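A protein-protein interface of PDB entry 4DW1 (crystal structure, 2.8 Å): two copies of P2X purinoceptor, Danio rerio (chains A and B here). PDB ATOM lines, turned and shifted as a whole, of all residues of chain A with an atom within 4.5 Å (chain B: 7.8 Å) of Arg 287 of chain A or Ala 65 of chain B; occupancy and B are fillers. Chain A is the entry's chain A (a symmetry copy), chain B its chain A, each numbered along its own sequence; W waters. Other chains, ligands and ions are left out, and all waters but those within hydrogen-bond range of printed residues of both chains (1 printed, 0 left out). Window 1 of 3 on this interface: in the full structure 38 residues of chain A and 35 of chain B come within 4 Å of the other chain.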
ATOM      1  N   THR A  86      22.956 -15.554   8.576  1.00  0.00           N
ATOM      2  CA  THR A  86      22.282 -15.586   9.866  1.00  0.00           C
ATOM      3  C   THR A  86      22.875 -16.702  10.695  1.00  0.00           C
ATOM      4  O   THR A  86      22.780 -17.865  10.324  1.00  0.00           O
ATOM      5  CB  THR A  86      20.794 -15.837   9.670  1.00  0.00           C
ATOM      6  OG1 THR A  86      20.262 -14.781   8.874  1.00  0.00           O
ATOM      7  CG2 THR A  86      20.079 -15.877  10.974  1.00  0.00           C
ATOM      8  N   THR A  87      23.461 -16.362  11.833  1.00  0.00           N
ATOM      9  CA  THR A  87      24.231 -17.349  12.570  1.00  0.00           C
ATOM     10  C   THR A  87      23.574 -17.665  13.889  1.00  0.00           C
ATOM     11  O   THR A  87      22.741 -16.911  14.377  1.00  0.00           O
ATOM     12  CB  THR A  87      25.695 -16.901  12.846  1.00  0.00           C
ATOM     13  OG1 THR A  87      25.699 -15.802  13.762  1.00  0.00           O
ATOM     14  CG2 THR A  87      26.415 -16.497  11.557  1.00  0.00           C
ATOM     15  N   ASN A  88      23.927 -18.822  14.420  1.00  0.00           N
ATOM     16  CA  ASN A  88      23.469 -19.223  15.717  1.00  0.00           C
ATOM     17  C   ASN A  88      21.971 -19.490  15.751  1.00  0.00           C
ATOM     18  O   ASN A  88      21.309 -19.220  16.740  1.00  0.00           O
ATOM     19  CB  ASN A  88      23.862 -18.151  16.716  1.00  0.00           C
ATOM     20  CG  ASN A  88      23.769 -18.615  18.122  1.00  0.00           C
ATOM     21  OD1 ASN A  88      24.053 -19.770  18.441  1.00  0.00           O
ATOM     22  ND2 ASN A  88      23.375 -17.715  19.001  1.00  0.00           N
ATOM     23  N   GLN A  89      21.451 -20.059  14.667  1.00  0.00           N
ATOM     24  CA  GLN A  89      20.067 -20.533  14.627  1.00  0.00           C
ATOM     25  C   GLN A  89      19.874 -21.839  15.379  1.00  0.00           C
ATOM     26  O   GLN A  89      20.763 -22.677  15.408  1.00  0.00           O
ATOM     27  CB  GLN A  89      19.588 -20.702  13.186  1.00  0.00           C
ATOM     28  CG  GLN A  89      19.330 -19.376  12.496  1.00  0.00           C
ATOM     29  CD  GLN A  89      18.680 -19.540  11.140  1.00  0.00           C
ATOM     30  OE1 GLN A  89      18.770 -20.607  10.528  1.00  0.00           O
ATOM     31  NE2 GLN A  89      18.016 -18.487  10.661  1.00  0.00           N
ATOM     32  N   TRP A 142      13.687 -22.020  12.779  1.00  0.00           N
ATOM     33  CA  TRP A 142      15.089 -21.817  13.097  1.00  0.00           C
ATOM     34  C   TRP A 142      15.231 -20.332  13.449  1.00  0.00           C
ATOM     35  O   TRP A 142      15.173 -19.452  12.586  1.00  0.00           O
ATOM     36  CB  TRP A 142      15.967 -22.111  11.891  1.00  0.00           C
ATOM     37  CG  TRP A 142      16.130 -23.566  11.523  1.00  0.00           C
ATOM     38  CD1 TRP A 142      15.504 -24.224  10.508  1.00  0.00           C
ATOM     39  CD2 TRP A 142      17.022 -24.516  12.123  1.00  0.00           C
ATOM     40  NE1 TRP A 142      15.933 -25.519  10.445  1.00  0.00           N
ATOM     41  CE2 TRP A 142      16.865 -25.729  11.428  1.00  0.00           C
ATOM     42  CE3 TRP A 142      17.936 -24.460  13.184  1.00  0.00           C
ATOM     43  CZ2 TRP A 142      17.589 -26.880  11.757  1.00  0.00           C
ATOM     44  CZ3 TRP A 142      18.651 -25.600  13.509  1.00  0.00           C
ATOM     45  CH2 TRP A 142      18.476 -26.791  12.801  1.00  0.00           C
ATOM     46  N   PHE A 274      21.372 -22.041   1.921  1.00  0.00           N
ATOM     47  CA  PHE A 274      21.940 -23.303   2.339  1.00  0.00           C
ATOM     48  C   PHE A 274      22.440 -23.072   3.734  1.00  0.00           C
ATOM     49  O   PHE A 274      22.401 -21.933   4.207  1.00  0.00           O
ATOM     50  CB  PHE A 274      23.055 -23.762   1.391  1.00  0.00           C
ATOM     51  CG  PHE A 274      24.251 -22.850   1.366  1.00  0.00           C
ATOM     52  CD1 PHE A 274      24.218 -21.658   0.648  1.00  0.00           C
ATOM     53  CD2 PHE A 274      25.413 -23.181   2.072  1.00  0.00           C
ATOM     54  CE1 PHE A 274      25.322 -20.795   0.633  1.00  0.00           C
ATOM     55  CE2 PHE A 274      26.522 -22.336   2.065  1.00  0.00           C
ATOM     56  CZ  PHE A 274      26.485 -21.138   1.343  1.00  0.00           C
ATOM     57  N   ALA A 275      22.919 -24.126   4.393  1.00  0.00           N
ATOM     58  CA  ALA A 275      23.232 -24.012   5.819  1.00  0.00           C
ATOM     59  C   ALA A 275      24.444 -24.831   6.224  1.00  0.00           C
ATOM     60  O   ALA A 275      24.878 -25.719   5.505  1.00  0.00           O
ATOM     61  CB  ALA A 275      22.018 -24.392   6.677  1.00  0.00           C
ATOM     62  N   LYS A 276      24.997 -24.500   7.376  1.00  0.00           N
ATOM     63  CA  LYS A 276      26.037 -25.308   7.955  1.00  0.00           C
ATOM     64  C   LYS A 276      25.582 -25.666   9.348  1.00  0.00           C
ATOM     65  O   LYS A 276      25.296 -24.767  10.144  1.00  0.00           O
ATOM     66  CB  LYS A 276      27.364 -24.554   7.979  1.00  0.00           C
ATOM     67  CG  LYS A 276      27.890 -24.312   6.592  1.00  0.00           C
ATOM     68  CD  LYS A 276      29.387 -24.034   6.577  1.00  0.00           C
ATOM     69  CE  LYS A 276      29.745 -22.798   7.394  1.00  0.00           C
ATOM     70  NZ  LYS A 276      31.191 -22.425   7.245  1.00  0.00           N
ATOM     71  N   TYR A 277      25.496 -26.970   9.627  1.00  0.00           N
ATOM     72  CA  TYR A 277      25.016 -27.464  10.915  1.00  0.00           C
ATOM     73  C   TYR A 277      26.147 -27.816  11.882  1.00  0.00           C
ATOM     74  O   TYR A 277      27.197 -28.296  11.462  1.00  0.00           O
ATOM     75  CB  TYR A 277      24.091 -28.659  10.705  1.00  0.00           C
ATOM     76  CG  TYR A 277      22.970 -28.380   9.740  1.00  0.00           C
ATOM     77  CD1 TYR A 277      23.177 -28.470   8.365  1.00  0.00           C
ATOM     78  CD2 TYR A 277      21.705 -28.004  10.197  1.00  0.00           C
ATOM     79  CE1 TYR A 277      22.156 -28.201   7.467  1.00  0.00           C
ATOM     80  CE2 TYR A 277      20.684 -27.734   9.313  1.00  0.00           C
ATOM     81  CZ  TYR A 277      20.915 -27.839   7.944  1.00  0.00           C
ATOM     82  OH  TYR A 277      19.898 -27.577   7.051  1.00  0.00           O
ATOM     83  N   THR A 286      22.826 -26.297  16.175  1.00  0.00           N
ATOM     84  CA  THR A 286      22.712 -24.907  15.769  1.00  0.00           C
ATOM     85  C   THR A 286      23.116 -24.806  14.303  1.00  0.00           C
ATOM     86  O   THR A 286      23.813 -25.671  13.769  1.00  0.00           O
ATOM     87  CB  THR A 286      23.566 -23.975  16.615  1.00  0.00           C
ATOM     88  OG1 THR A 286      24.906 -24.006  16.120  1.00  0.00           O
ATOM     89  CG2 THR A 286      23.556 -24.413  18.068  1.00  0.00           C
ATOM     90  N   ARG A 287      22.690 -23.741  13.647  1.00  0.00           N
ATOM     91  CA  ARG A 287      22.760 -23.705  12.208  1.00  0.00           C
ATOM     92  C   ARG A 287      23.198 -22.330  11.749  1.00  0.00           C
ATOM     93  O   ARG A 287      22.807 -21.326  12.330  1.00  0.00           O
ATOM     94  CB  ARG A 287      21.368 -23.999  11.672  1.00  0.00           C
ATOM     95  CG  ARG A 287      21.292 -24.279  10.199  1.00  0.00           C
ATOM     96  CD  ARG A 287      19.869 -24.640   9.806  1.00  0.00           C
ATOM     97  NE  ARG A 287      19.072 -23.462   9.501  1.00  0.00           N
ATOM     98  CZ  ARG A 287      18.090 -23.452   8.607  1.00  0.00           C
ATOM     99  NH1 ARG A 287      17.793 -24.562   7.941  1.00  0.00           N
ATOM    100  NH2 ARG A 287      17.423 -22.331   8.369  1.00  0.00           N
ATOM    101  N   THR A 288      24.021 -22.277  10.711  1.00  0.00           N
ATOM    102  CA  THR A 288      24.270 -21.014  10.041  1.00  0.00           C
ATOM    103  C   THR A 288      23.558 -21.062   8.714  1.00  0.00           C
ATOM    104  O   THR A 288      23.783 -21.966   7.902  1.00  0.00           O
ATOM    105  CB  THR A 288      25.754 -20.784   9.793  1.00  0.00           C
ATOM    106  OG1 THR A 288      26.414 -20.635  11.048  1.00  0.00           O
ATOM    107  CG2 THR A 288      25.976 -19.524   8.934  1.00  0.00           C
ATOM    108  N   LEU A 289      22.678 -20.103   8.497  1.00  0.00           N
ATOM    109  CA  LEU A 289      21.953 -20.039   7.240  1.00  0.00           C
ATOM    110  C   LEU A 289      22.561 -18.933   6.383  1.00  0.00           C
ATOM    111  O   LEU A 289      22.785 -17.833   6.861  1.00  0.00           O
ATOM    112  CB  LEU A 289      20.474 -19.796   7.510  1.00  0.00           C
ATOM    113  CG  LEU A 289      19.534 -19.450   6.359  1.00  0.00           C
ATOM    114  CD1 LEU A 289      19.109 -20.690   5.586  1.00  0.00           C
ATOM    115  CD2 LEU A 289      18.327 -18.715   6.926  1.00  0.00           C
ATOM    116  N   VAL B  46      12.522 -23.068  -3.803  1.00  0.00           N
ATOM    117  CA  VAL B  46      11.395 -23.734  -3.211  1.00  0.00           C
ATOM    118  C   VAL B  46      11.162 -23.052  -1.883  1.00  0.00           C
ATOM    119  O   VAL B  46      12.105 -22.618  -1.238  1.00  0.00           O
ATOM    120  CB  VAL B  46      11.642 -25.276  -3.064  1.00  0.00           C
ATOM    121  CG1 VAL B  46      10.592 -25.926  -2.144  1.00  0.00           C
ATOM    122  CG2 VAL B  46      11.652 -25.938  -4.438  1.00  0.00           C
ATOM    123  N   GLY B  48       8.689 -23.157   1.803  1.00  0.00           N
ATOM    124  CA  GLY B  48       7.716 -23.885   2.585  1.00  0.00           C
ATOM    125  C   GLY B  48       8.374 -24.421   3.828  1.00  0.00           C
ATOM    126  O   GLY B  48       9.607 -24.408   3.929  1.00  0.00           O
ATOM    127  N   ARG B  60      10.289 -30.862  15.253  1.00  0.00           N
ATOM    128  CA  ARG B  60      11.343 -30.250  14.463  1.00  0.00           C
ATOM    129  C   ARG B  60      10.735 -29.637  13.196  1.00  0.00           C
ATOM    130  O   ARG B  60       9.796 -30.196  12.628  1.00  0.00           O
ATOM    131  CB  ARG B  60      12.390 -31.334  14.126  1.00  0.00           C
ATOM    132  CG  ARG B  60      13.488 -30.915  13.172  1.00  0.00           C
ATOM    133  CD  ARG B  60      14.828 -31.542  13.568  1.00  0.00           C
ATOM    134  NE  ARG B  60      15.980 -31.252  12.690  1.00  0.00           N
ATOM    135  CZ  ARG B  60      15.935 -30.649  11.501  1.00  0.00           C
ATOM    136  NH1 ARG B  60      14.779 -30.228  10.994  1.00  0.00           N
ATOM    137  NH2 ARG B  60      17.067 -30.468  10.809  1.00  0.00           N
ATOM    138  N   ILE B  61      11.256 -28.489  12.765  1.00  0.00           N
ATOM    139  CA  ILE B  61      10.910 -27.947  11.450  1.00  0.00           C
ATOM    140  C   ILE B  61      11.998 -28.207  10.416  1.00  0.00           C
ATOM    141  O   ILE B  61      13.178 -28.291  10.727  1.00  0.00           O
ATOM    142  CB  ILE B  61      10.669 -26.421  11.448  1.00  0.00           C
ATOM    143  CG1 ILE B  61      11.951 -25.692  11.846  1.00  0.00           C
ATOM    144  CG2 ILE B  61       9.476 -26.024  12.308  1.00  0.00           C
ATOM    145  CD1 ILE B  61      12.128 -24.392  11.122  1.00  0.00           C
ATOM    146  N   TRP B  62      11.566 -28.352   9.178  1.00  0.00           N
ATOM    147  CA  TRP B  62      12.441 -28.482   8.039  1.00  0.00           C
ATOM    148  C   TRP B  62      12.137 -27.345   7.092  1.00  0.00           C
ATOM    149  O   TRP B  62      11.007 -27.233   6.597  1.00  0.00           O
ATOM    150  CB  TRP B  62      12.179 -29.814   7.357  1.00  0.00           C
ATOM    151  CG  TRP B  62      12.460 -30.938   8.288  1.00  0.00           C
ATOM    152  CD1 TRP B  62      11.769 -31.251   9.421  1.00  0.00           C
ATOM    153  CD2 TRP B  62      13.530 -31.879   8.193  1.00  0.00           C
ATOM    154  NE1 TRP B  62      12.339 -32.339  10.033  1.00  0.00           N
ATOM    155  CE2 TRP B  62      13.425 -32.738   9.303  1.00  0.00           C
ATOM    156  CE3 TRP B  62      14.562 -32.083   7.276  1.00  0.00           C
ATOM    157  CZ2 TRP B  62      14.312 -33.780   9.520  1.00  0.00           C
ATOM    158  CZ3 TRP B  62      15.442 -33.118   7.492  1.00  0.00           C
ATOM    159  CH2 TRP B  62      15.309 -33.957   8.603  1.00  0.00           C
ATOM    160  N   ASP B  63      13.141 -26.501   6.834  1.00  0.00           N
ATOM    161  CA  ASP B  63      12.967 -25.440   5.859  1.00  0.00           C
ATOM    162  C   ASP B  63      13.819 -25.710   4.631  1.00  0.00           C
ATOM    163  O   ASP B  63      14.408 -26.772   4.518  1.00  0.00           O
ATOM    164  CB  ASP B  63      13.196 -24.045   6.452  1.00  0.00           C
ATOM    165  CG  ASP B  63      14.656 -23.727   6.661  1.00  0.00           C
ATOM    166  OD1 ASP B  63      15.506 -24.349   5.988  1.00  0.00           O
ATOM    167  OD2 ASP B  63      14.951 -22.831   7.485  1.00  0.00           O
ATOM    168  N   VAL B  64      13.835 -24.761   3.696  1.00  0.00           N
ATOM    169  CA  VAL B  64      14.455 -24.953   2.388  1.00  0.00           C
ATOM    170  C   VAL B  64      15.894 -25.471   2.484  1.00  0.00           C
ATOM    171  O   VAL B  64      16.337 -26.246   1.640  1.00  0.00           O
ATOM    172  CB  VAL B  64      14.452 -23.629   1.585  1.00  0.00           C
ATOM    173  CG1 VAL B  64      15.478 -22.685   2.133  1.00  0.00           C
ATOM    174  CG2 VAL B  64      14.722 -23.878   0.123  1.00  0.00           C
ATOM    175  N   ALA B  65      16.629 -25.036   3.505  1.00  0.00           N
ATOM    176  CA  ALA B  65      18.031 -25.411   3.626  1.00  0.00           C
ATOM    177  C   ALA B  65      18.157 -26.823   4.198  1.00  0.00           C
ATOM    178  O   ALA B  65      19.212 -27.439   4.111  1.00  0.00           O
ATOM    179  CB  ALA B  65      18.770 -24.405   4.496  1.00  0.00           C
ATOM    180  N   ASP B  66      17.084 -27.303   4.815  1.00  0.00           N
ATOM    181  CA  ASP B  66      16.996 -28.654   5.323  1.00  0.00           C
ATOM    182  C   ASP B  66      16.590 -29.675   4.273  1.00  0.00           C
ATOM    183  O   ASP B  66      17.099 -30.792   4.274  1.00  0.00           O
ATOM    184  CB  ASP B  66      15.996 -28.720   6.470  1.00  0.00           C
ATOM    185  CG  ASP B  66      16.355 -27.805   7.600  1.00  0.00           C
ATOM    186  OD1 ASP B  66      15.448 -27.183   8.173  1.00  0.00           O
ATOM    187  OD2 ASP B  66      17.551 -27.685   7.907  1.00  0.00           O
ATOM    188  N   TYR B  67      15.609 -29.326   3.445  1.00  0.00           N
ATOM    189  CA  TYR B  67      15.001 -30.286   2.512  1.00  0.00           C
ATOM    190  C   TYR B  67      15.405 -30.232   1.012  1.00  0.00           C
ATOM    191  O   TYR B  67      14.943 -31.056   0.208  1.00  0.00           O
ATOM    192  CB  TYR B  67      13.465 -30.333   2.698  1.00  0.00           C
ATOM    193  CG  TYR B  67      12.736 -29.027   2.452  1.00  0.00           C
ATOM    194  CD1 TYR B  67      12.659 -28.496   1.172  1.00  0.00           C
ATOM    195  CD2 TYR B  67      12.113 -28.337   3.492  1.00  0.00           C
ATOM    196  CE1 TYR B  67      12.014 -27.318   0.926  1.00  0.00           C
ATOM    197  CE2 TYR B  67      11.434 -27.139   3.255  1.00  0.00           C
ATOM    198  CZ  TYR B  67      11.399 -26.642   1.957  1.00  0.00           C
ATOM    199  OH  TYR B  67      10.755 -25.474   1.652  1.00  0.00           O
ATOM    200  N   ILE B  68      16.238 -29.278   0.611  1.00  0.00           N
ATOM    201  CA  ILE B  68      16.716 -29.337  -0.768  1.00  0.00           C
ATOM    202  C   ILE B  68      18.160 -29.833  -0.811  1.00  0.00           C
ATOM    203  O   ILE B  68      19.079 -29.123  -0.405  1.00  0.00           O
ATOM    204  CB  ILE B  68      16.617 -27.995  -1.484  1.00  0.00           C
ATOM    205  CG1 ILE B  68      15.239 -27.371  -1.270  1.00  0.00           C
ATOM    206  CG2 ILE B  68      16.872 -28.184  -2.976  1.00  0.00           C
ATOM    207  CD1 ILE B  68      14.080 -28.182  -1.885  1.00  0.00           C
ATOM    208  N   ILE B  69      18.350 -31.063  -1.283  1.00  0.00           N
ATOM    209  CA  ILE B  69      19.679 -31.663  -1.364  1.00  0.00           C
ATOM    210  C   ILE B  69      20.065 -31.987  -2.794  1.00  0.00           C
ATOM    211  O   ILE B  69      19.465 -32.849  -3.418  1.00  0.00           O
ATOM    212  CB  ILE B  69      19.744 -32.997  -0.616  1.00  0.00           C
ATOM    213  CG1 ILE B  69      18.750 -33.054   0.562  1.00  0.00           C
ATOM    214  CG2 ILE B  69      21.163 -33.322  -0.255  1.00  0.00           C
ATOM    215  CD1 ILE B  69      18.838 -31.940   1.517  1.00  0.00           C
ATOM    216  N   PRO B  70      21.069 -31.303  -3.336  1.00  0.00           N
ATOM    217  CA  PRO B  70      21.799 -30.184  -2.749  1.00  0.00           C
ATOM    218  C   PRO B  70      21.028 -28.883  -2.987  1.00  0.00           C
ATOM    219  O   PRO B  70      19.959 -28.899  -3.596  1.00  0.00           O
ATOM    220  CB  PRO B  70      23.110 -30.208  -3.535  1.00  0.00           C
ATOM    221  CG  PRO B  70      22.731 -30.722  -4.871  1.00  0.00           C
ATOM    222  CD  PRO B  70      21.615 -31.692  -4.650  1.00  0.00           C
ATOM    223  N   PRO B  71      21.569 -27.754  -2.520  1.00  0.00           N
ATOM    224  CA  PRO B  71      20.844 -26.486  -2.597  1.00  0.00           C
ATOM    225  C   PRO B  71      20.642 -26.028  -4.024  1.00  0.00           C
ATOM    226  O   PRO B  71      19.731 -25.255  -4.303  1.00  0.00           O
ATOM    227  CB  PRO B  71      21.797 -25.512  -1.916  1.00  0.00           C
ATOM    228  CG  PRO B  71      22.738 -26.361  -1.137  1.00  0.00           C
ATOM    229  CD  PRO B  71      22.899 -27.588  -1.921  1.00  0.00           C
ATOM    230  N   LYS B 276      25.389 -35.893   8.078  1.00  0.00           N
ATOM    231  CA  LYS B 276      25.840 -34.656   8.653  1.00  0.00           C
ATOM    232  C   LYS B 276      26.873 -35.014   9.693  1.00  0.00           C
ATOM    233  O   LYS B 276      26.573 -35.784  10.609  1.00  0.00           O
ATOM    234  CB  LYS B 276      24.676 -33.883   9.269  1.00  0.00           C
ATOM    235  CG  LYS B 276      23.710 -33.407   8.220  1.00  0.00           C
ATOM    236  CD  LYS B 276      22.848 -32.250   8.705  1.00  0.00           C
ATOM    237  CE  LYS B 276      22.010 -32.633   9.919  1.00  0.00           C
ATOM    238  NZ  LYS B 276      21.039 -31.552  10.296  1.00  0.00           N
HETATM  239  O   HOH W   1      21.929 -26.699   3.059  1.00  0.00           O
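OD2 of Asp 63 of chain B is in salt-bridge range of NH2 of Arg 287 of chain A, at 2.7 Å. The side-chain hydroxyl (OH) of Tyr 277 of chain A is in hydrogen-bond range of the backbone carbonyl oxygen (O) of Ala 65 of chain B (3.0 Å). The side-chain carboxylate of Asp 66 of chain B is in hydrogen-bond range of the indole nitrogen of Trp 142 of chain A. The side-chain carboxylate of Asp 66 of chain B lies within hydrogen-bond range of the side-chain hydroxyl of Tyr 277 of chain A (2.5 Å). OD2 of Asp 66 of chain B is in salt-bridge range of NH1 of Arg 287 of chain A (3.1 Å).
The side-chain carboxylate (OD1) of Asp 63 of chain B sits at hydrogen-bond distance from the backbone NH (N) of Ala 65 of chain B (2.8 Å). N of Asp 63 of chain B is in hydrogen-bond range of OD1 of Asp 66 of chain B (2.8 Å). N of Thr 86 of chain A sits at hydrogen-bond distance from O of Leu 289 of chain A (2.9 Å). The backbone carbonyl oxygen (O) of Arg 287 of chain A lies within hydrogen-bond range of the backbone NH (N) of Asn 88 of chain A (3.4 Å). The backbone carbonyl oxygen (O) of Gln 89 of chain A lies within hydrogen-bond range of the backbone NH (N) of Arg 287 of chain A (2.8 Å).
Arg 60 of chain B touches Trp 142 of chain A (NH2 to CZ2, 3.7 Å). Ile 61 of chain B touches Trp 142 of chain A. Asp 63 of chain B touches Trp 142 of chain A (OD2 to CD1, 3.4 Å). Phe 274 of chain A touches Ala 65 of chain B (C to CB, 3.98 Å). Pro 71 of chain B touches Phe 274 of chain A. Ala 275 of chain A touches Ala 65 of chain B. Tyr 277 of chain A touches Lys 276 of chain B (CD2 to NZ, 3.6 Å). Arg 287 of chain A touches Ala 65 of chain B (NH1 to CB, 3.6 Å). Leu 289 of chain A touches Ala 65 of chain B.
Of the printed residues of chain B, Tyr 277 of chain A touches Ala 65, Asp 66 and Lys 276. Arg 287 of chain A touches just these residues of chain B: Asp 63 (2.7 Å), Ala 65 (3.6 Å) and Asp 66 (3.1 Å). Of the printed residues of chain B, Leu 289 of chain A touches Ala 65. Printed residues of chain A within 4 Å of Arg 60 of chain B: Trp 142. Of the printed residues of chain A, Ile 61 of chain B touches Trp 142 (3.3 Å). Of chain A, only Phe 274 (3.98 Å), Ala 275 (3.9 Å), Tyr 277 (3.0 Å), Arg 287 (3.6 Å) and Leu 289 (3.9 Å) come within 4 Å of Ala 65 of chain B. The nearest residue of chain B that does not touch Arg 287 of chain A is Val 64 of chain B (5.8 Å). The nearest printed residue of chain A that does not touch Ala 65 of chain B is Thr 288 of chain A (6.5 Å).
Of the 15 printed residues of chain B, 7 touch a printed residue of chain A. Printed residues of chain B that touch a printed residue of chain A: Arg 60, Ile 61, Asp 63, Ala 65, Asp 66, Pro 71 and Lys 276. Hydrophobic or aromatic side chains of chain B that line the printed part of chain A: Ile 61, Ala 65 and Pro 71. Hydrophobic or aromatic side chains of chain A within 4 Å of the printed part of chain B: Trp 142, Phe 274, Ala 275, Tyr 277 and Leu 289. Among the printed residues, 14 pairs touch across the chains.
Position printed for both chains: 276. Of the 14 pairs that touch across the chains among the printed residues, none has its exchanged pair printed and touching as well.
Water W1 bridges O of Ala 65 of chain B (3.0 Å) and N of Ala 275 of chain A (3.1 Å).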
